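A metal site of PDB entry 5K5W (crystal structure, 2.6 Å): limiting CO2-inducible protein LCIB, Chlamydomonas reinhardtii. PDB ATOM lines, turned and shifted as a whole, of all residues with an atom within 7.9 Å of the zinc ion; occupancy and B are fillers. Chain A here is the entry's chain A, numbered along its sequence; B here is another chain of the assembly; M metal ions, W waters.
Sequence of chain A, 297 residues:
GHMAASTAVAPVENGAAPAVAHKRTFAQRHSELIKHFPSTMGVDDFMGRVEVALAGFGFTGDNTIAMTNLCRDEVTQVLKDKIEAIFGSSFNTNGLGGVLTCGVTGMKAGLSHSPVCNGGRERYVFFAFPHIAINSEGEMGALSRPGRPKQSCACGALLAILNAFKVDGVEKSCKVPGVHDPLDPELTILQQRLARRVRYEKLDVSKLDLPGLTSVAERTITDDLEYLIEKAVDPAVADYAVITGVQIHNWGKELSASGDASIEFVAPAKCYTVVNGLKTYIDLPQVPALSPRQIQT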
ATOM      1  N   LEU A  70      -8.834  -7.630  28.489  1.00  0.00           N
ATOM      2  CA  LEU A  70      -7.487  -7.109  28.321  1.00  0.00           C
ATOM      3  C   LEU A  70      -7.592  -5.602  28.340  1.00  0.00           C
ATOM      4  O   LEU A  70      -8.686  -5.058  28.504  1.00  0.00           O
ATOM      5  CB  LEU A  70      -6.852  -7.583  27.009  1.00  0.00           C
ATOM      6  CG  LEU A  70      -6.774  -9.091  26.820  1.00  0.00           C
ATOM      7  CD1 LEU A  70      -6.449  -9.427  25.370  1.00  0.00           C
ATOM      8  CD2 LEU A  70      -5.718  -9.631  27.769  1.00  0.00           C
ATOM      9  N   CYS A  71      -6.442  -4.956  28.171  1.00  0.00           N
ATOM     10  CA  CYS A  71      -6.383  -3.521  27.939  1.00  0.00           C
ATOM     11  C   CYS A  71      -6.917  -3.158  26.534  1.00  0.00           C
ATOM     12  O   CYS A  71      -6.705  -3.900  25.566  1.00  0.00           O
ATOM     13  CB  CYS A  71      -4.948  -3.030  28.113  1.00  0.00           C
ATOM     14  SG  CYS A  71      -4.784  -1.244  27.995  1.00  0.00           S
ATOM     15  N   ARG A  72      -7.603  -2.020  26.446  1.00  0.00           N
ATOM     16  CA  ARG A  72      -8.147  -1.536  25.179  1.00  0.00           C
ATOM     17  C   ARG A  72      -7.070  -1.357  24.125  1.00  0.00           C
ATOM     18  O   ARG A  72      -7.336  -1.488  22.939  1.00  0.00           O
ATOM     19  CB  ARG A  72      -8.897  -0.208  25.363  1.00  0.00           C
ATOM     20  CG  ARG A  72     -10.249  -0.352  26.083  1.00  0.00           C
ATOM     21  CD  ARG A  72     -11.086   0.910  25.966  1.00  0.00           C
ATOM     22  NE  ARG A  72     -12.287   0.897  26.801  1.00  0.00           N
ATOM     23  CZ  ARG A  72     -13.480   0.451  26.406  1.00  0.00           C
ATOM     24  NH1 ARG A  72     -13.651  -0.025  25.181  1.00  0.00           N
ATOM     25  NH2 ARG A  72     -14.503   0.484  27.247  1.00  0.00           N
ATOM     26  N   ASP A  73      -5.861  -1.037  24.551  1.00  0.00           N
ATOM     27  CA  ASP A  73      -4.766  -0.786  23.643  1.00  0.00           C
ATOM     28  C   ASP A  73      -4.707  -1.791  22.552  1.00  0.00           C
ATOM     29  O   ASP A  73      -5.073  -2.891  22.760  1.00  0.00           O
ATOM     30  CB  ASP A  73      -3.452  -0.800  24.395  1.00  0.00           C
ATOM     31  CG  ASP A  73      -2.377  -0.023  23.694  1.00  0.00           C
ATOM     32  OD1 ASP A  73      -2.487   0.197  22.488  1.00  0.00           O
ATOM     33  OD2 ASP A  73      -1.417   0.383  24.329  1.00  0.00           O
ATOM     34  N   GLU A  74      -4.258  -1.407  21.370  1.00  0.00           N
ATOM     35  CA  GLU A  74      -4.183  -2.375  20.310  1.00  0.00           C
ATOM     36  C   GLU A  74      -3.277  -3.527  20.500  1.00  0.00           C
ATOM     37  O   GLU A  74      -3.607  -4.619  20.129  1.00  0.00           O
ATOM     38  CB  GLU A  74      -3.787  -1.693  19.017  1.00  0.00           C
ATOM     39  CG  GLU A  74      -4.157  -0.229  18.918  1.00  0.00           C
ATOM     40  CD  GLU A  74      -3.063   0.593  18.309  1.00  0.00           C
ATOM     41  OE1 GLU A  74      -1.886   0.321  18.619  1.00  0.00           O
ATOM     42  OE2 GLU A  74      -3.382   1.508  17.537  1.00  0.00           O
ATOM     43  N   VAL A  75      -2.129  -3.293  21.045  1.00  0.00           N
ATOM     44  CA  VAL A  75      -1.162  -4.379  21.154  1.00  0.00           C
ATOM     45  C   VAL A  75      -1.653  -5.606  21.923  1.00  0.00           C
ATOM     46  O   VAL A  75      -0.985  -6.635  21.889  1.00  0.00           O
ATOM     47  CB  VAL A  75       0.138  -3.897  21.807  1.00  0.00           C
ATOM     48  CG1 VAL A  75       0.743  -2.785  20.988  1.00  0.00           C
ATOM     49  CG2 VAL A  75      -0.137  -3.420  23.235  1.00  0.00           C
ATOM     50  N   THR A  76      -2.786  -5.524  22.604  1.00  0.00           N
ATOM     51  CA  THR A  76      -3.278  -6.673  23.378  1.00  0.00           C
ATOM     52  C   THR A  76      -3.952  -7.729  22.499  1.00  0.00           C
ATOM     53  O   THR A  76      -4.244  -8.836  22.968  1.00  0.00           O
ATOM     54  CB  THR A  76      -4.272  -6.248  24.494  1.00  0.00           C
ATOM     55  OG1 THR A  76      -5.197  -5.261  23.998  1.00  0.00           O
ATOM     56  CG2 THR A  76      -3.524  -5.668  25.670  1.00  0.00           C
ATOM     57  N   GLY A  95     -11.176  -2.792  28.968  1.00  0.00           N
ATOM     58  CA  GLY A  95     -11.178  -1.442  29.497  1.00  0.00           C
ATOM     59  C   GLY A  95      -9.762  -0.875  29.582  1.00  0.00           C
ATOM     60  O   GLY A  95      -8.789  -1.567  29.279  1.00  0.00           O
ATOM     61  N   LEU A  96      -9.616   0.393  29.958  1.00  0.00           N
ATOM     62  CA  LEU A  96      -8.263   0.931  30.132  1.00  0.00           C
ATOM     63  C   LEU A  96      -7.495   0.143  31.196  1.00  0.00           C
ATOM     64  O   LEU A  96      -8.003  -0.109  32.289  1.00  0.00           O
ATOM     65  CB  LEU A  96      -8.300   2.415  30.500  1.00  0.00           C
ATOM     66  CG  LEU A  96      -7.671   3.330  29.452  1.00  0.00           C
ATOM     67  CD1 LEU A  96      -8.341   3.078  28.111  1.00  0.00           C
ATOM     68  CD2 LEU A  96      -7.757   4.810  29.860  1.00  0.00           C
ATOM     69  N   GLY A  97      -6.276  -0.273  30.829  1.00  0.00           N
ATOM     70  CA  GLY A  97      -5.402  -1.093  31.678  1.00  0.00           C
ATOM     71  C   GLY A  97      -5.939  -2.457  32.099  1.00  0.00           C
ATOM     72  O   GLY A  97      -5.276  -3.175  32.859  1.00  0.00           O
ATOM     73  N   GLY A  98      -7.126  -2.843  31.622  1.00  0.00           N
ATOM     74  CA  GLY A  98      -7.718  -4.116  31.999  1.00  0.00           C
ATOM     75  C   GLY A  98      -8.753  -4.017  33.113  1.00  0.00           C
ATOM     76  O   GLY A  98      -9.135  -5.035  33.715  1.00  0.00           O
ATOM     77  N   PRO A 130      -3.697  -7.725  32.608  1.00  0.00           N
ATOM     78  CA  PRO A 130      -3.063  -6.461  32.205  1.00  0.00           C
ATOM     79  C   PRO A 130      -1.858  -6.754  31.302  1.00  0.00           C
ATOM     80  O   PRO A 130      -1.663  -7.901  30.877  1.00  0.00           O
ATOM     81  CB  PRO A 130      -2.651  -5.841  33.536  1.00  0.00           C
ATOM     82  CG  PRO A 130      -2.415  -7.014  34.417  1.00  0.00           C
ATOM     83  CD  PRO A 130      -3.388  -8.079  33.996  1.00  0.00           C
ATOM     84  N   HIS A 131      -1.052  -5.739  31.002  1.00  0.00           N
ATOM     85  CA  HIS A 131       0.108  -5.940  30.140  1.00  0.00           C
ATOM     86  C   HIS A 131       1.215  -4.932  30.398  1.00  0.00           C
ATOM     87  O   HIS A 131       1.082  -4.037  31.236  1.00  0.00           O
ATOM     88  CB  HIS A 131      -0.308  -5.886  28.663  1.00  0.00           C
ATOM     89  CG  HIS A 131      -0.758  -4.527  28.213  1.00  0.00           C
ATOM     90  ND1 HIS A 131      -0.782  -4.165  26.882  1.00  0.00           N
ATOM     91  CD2 HIS A 131      -1.190  -3.453  28.911  1.00  0.00           C
ATOM     92  CE1 HIS A 131      -1.219  -2.919  26.786  1.00  0.00           C
ATOM     93  NE2 HIS A 131      -1.470  -2.473  27.994  1.00  0.00           N
ATOM     94  N   ILE A 132       2.312  -5.093  29.677  1.00  0.00           N
ATOM     95  CA  ILE A 132       3.461  -4.202  29.808  1.00  0.00           C
ATOM     96  C   ILE A 132       4.422  -4.460  28.636  1.00  0.00           C
ATOM     97  O   ILE A 132       4.387  -5.547  28.039  1.00  0.00           O
ATOM     98  CB  ILE A 132       4.167  -4.441  31.184  1.00  0.00           C
ATOM     99  CG1 ILE A 132       5.356  -3.501  31.407  1.00  0.00           C
ATOM    100  CG2 ILE A 132       4.597  -5.885  31.334  1.00  0.00           C
ATOM    101  CD1 ILE A 132       5.957  -3.622  32.780  1.00  0.00           C
ATOM    102  N   CYS A 153       6.111   2.133  25.206  1.00  0.00           N
ATOM    103  CA  CYS A 153       4.997   2.469  26.059  1.00  0.00           C
ATOM    104  C   CYS A 153       4.234   1.212  26.356  1.00  0.00           C
ATOM    105  O   CYS A 153       3.563   0.703  25.489  1.00  0.00           O
ATOM    106  CB  CYS A 153       4.135   3.418  25.284  1.00  0.00           C
ATOM    107  SG  CYS A 153       4.966   3.977  23.806  1.00  0.00           S
ATOM    108  N   ALA A 154       4.361   0.698  27.574  1.00  0.00           N
ATOM    109  CA  ALA A 154       3.684  -0.513  28.000  1.00  0.00           C
ATOM    110  C   ALA A 154       2.284  -0.128  28.123  1.00  0.00           C
ATOM    111  O   ALA A 154       1.728   0.437  27.218  1.00  0.00           O
ATOM    112  CB  ALA A 154       4.183  -0.923  29.355  1.00  0.00           C
ATOM    113  N   CYS A 155       1.682  -0.410  29.240  1.00  0.00           N
ATOM    114  CA  CYS A 155       0.319   0.068  29.419  1.00  0.00           C
ATOM    115  C   CYS A 155       0.395   1.529  29.823  1.00  0.00           C
ATOM    116  O   CYS A 155       0.721   1.841  30.985  1.00  0.00           O
ATOM    117  CB  CYS A 155      -0.456  -0.731  30.452  1.00  0.00           C
ATOM    118  SG  CYS A 155      -2.192  -0.258  30.462  1.00  0.00           S
ATOM    119  N   GLY A 156       0.116   2.409  28.866  1.00  0.00           N
ATOM    120  CA  GLY A 156       0.064   3.850  29.110  1.00  0.00           C
ATOM    121  C   GLY A 156      -0.753   4.210  30.331  1.00  0.00           C
ATOM    122  O   GLY A 156      -0.444   5.171  31.039  1.00  0.00           O
ATOM    123  N   ALA A 157      -1.789   3.417  30.597  1.00  0.00           N
ATOM    124  CA  ALA A 157      -2.672   3.601  31.746  1.00  0.00           C
ATOM    125  C   ALA A 157      -1.973   3.304  33.067  1.00  0.00           C
ATOM    126  O   ALA A 157      -2.019   4.106  34.004  1.00  0.00           O
ATOM    127  CB  ALA A 157      -3.909   2.720  31.596  1.00  0.00           C
ATOM    128  N   LEU A 158      -1.347   2.141  33.159  1.00  0.00           N
ATOM    129  CA  LEU A 158      -0.616   1.779  34.366  1.00  0.00           C
ATOM    130  C   LEU A 158       0.546   2.738  34.591  1.00  0.00           C
ATOM    131  O   LEU A 158       0.832   3.117  35.719  1.00  0.00           O
ATOM    132  CB  LEU A 158      -0.132   0.341  34.306  1.00  0.00           C
ATOM    133  CG  LEU A 158      -1.248  -0.696  34.405  1.00  0.00           C
ATOM    134  CD1 LEU A 158      -0.787  -2.086  33.949  1.00  0.00           C
ATOM    135  CD2 LEU A 158      -1.767  -0.725  35.825  1.00  0.00           C
ATOM    136  N   LEU A 159       1.201   3.168  33.513  1.00  0.00           N
ATOM    137  CA  LEU A 159       2.294   4.134  33.658  1.00  0.00           C
ATOM    138  C   LEU A 159       1.785   5.511  34.062  1.00  0.00           C
ATOM    139  O   LEU A 159       2.526   6.317  34.616  1.00  0.00           O
ATOM    140  CB  LEU A 159       3.106   4.250  32.386  1.00  0.00           C
ATOM    141  CG  LEU A 159       4.456   4.942  32.636  1.00  0.00           C
ATOM    142  CD1 LEU A 159       5.525   3.915  32.933  1.00  0.00           C
ATOM    143  CD2 LEU A 159       4.849   5.833  31.455  1.00  0.00           C
ATOM    144  N   HIS A 249       5.546  -7.833  26.234  1.00  0.00           N
ATOM    145  CA  HIS A 249       5.732  -7.687  24.797  1.00  0.00           C
ATOM    146  C   HIS A 249       7.127  -8.088  24.258  1.00  0.00           C
ATOM    147  O   HIS A 249       7.233  -9.031  23.454  1.00  0.00           O
ATOM    148  CB  HIS A 249       5.376  -6.250  24.412  1.00  0.00           C
ATOM    149  CG  HIS A 249       3.907  -5.956  24.560  1.00  0.00           C
ATOM    150  ND1 HIS A 249       2.925  -6.713  23.964  1.00  0.00           N
ATOM    151  CD2 HIS A 249       3.263  -5.006  25.284  1.00  0.00           C
ATOM    152  CE1 HIS A 249       1.735  -6.241  24.294  1.00  0.00           C
ATOM    153  NE2 HIS A 249       1.916  -5.202  25.094  1.00  0.00           N
ATOM    154  N   ALA B 109      -5.485   7.667  23.732  1.00  0.00           N
ATOM    155  CA  ALA B 109      -4.799   6.410  23.469  1.00  0.00           C
ATOM    156  C   ALA B 109      -5.021   5.935  22.018  1.00  0.00           C
ATOM    157  O   ALA B 109      -4.090   5.482  21.351  1.00  0.00           O
ATOM    158  CB  ALA B 109      -5.271   5.340  24.451  1.00  0.00           C
HETATM  159 ZN    ZN M   1      -2.550  -0.687  28.177  1.00  0.00          ZN
HETATM  160  O   HOH W   1      -1.594   1.081  26.682  1.00  0.00           O
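The side-chain sulfur of Cys 155 sits close to the backbone NH of Ala 157, at 3.7 Å. ND1 of His 131 lies within hydrogen-bond range of NE2 of His 249 (3.4 Å). O of Asp 73 sits at hydrogen-bond distance from OG1 of Thr 76 (2.7 Å). O of Cys 71 is in hydrogen-bond range of OG1 of Thr 76 (2.6 Å). The backbone NH (N) of Gly 97 lies close to the side-chain sulfur (SG) of Cys 71 (3.3 Å). SG of Cys 155 sits close to N of Leu 158, at 3.7 Å. The backbone NH of Asp 73 lies close to the side-chain sulfur of Cys 71.
Asp 73 touches the zinc ion. Within 4 Å of the zinc ion: Cys 71, Asp 73, His 131 and Cys 155.
The zinc ion is bound by NE2 of His 131, SG of Cys 71, SG of Cys 155 and water W1. The zinc ion has four donor atoms within binding distance.
Water W1 lies within hydrogen-bond range of OD2 of Asp 73 (2.5 Å), N of Gly 156 (3.1 Å) and O of Ala 154 (3.4 Å).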
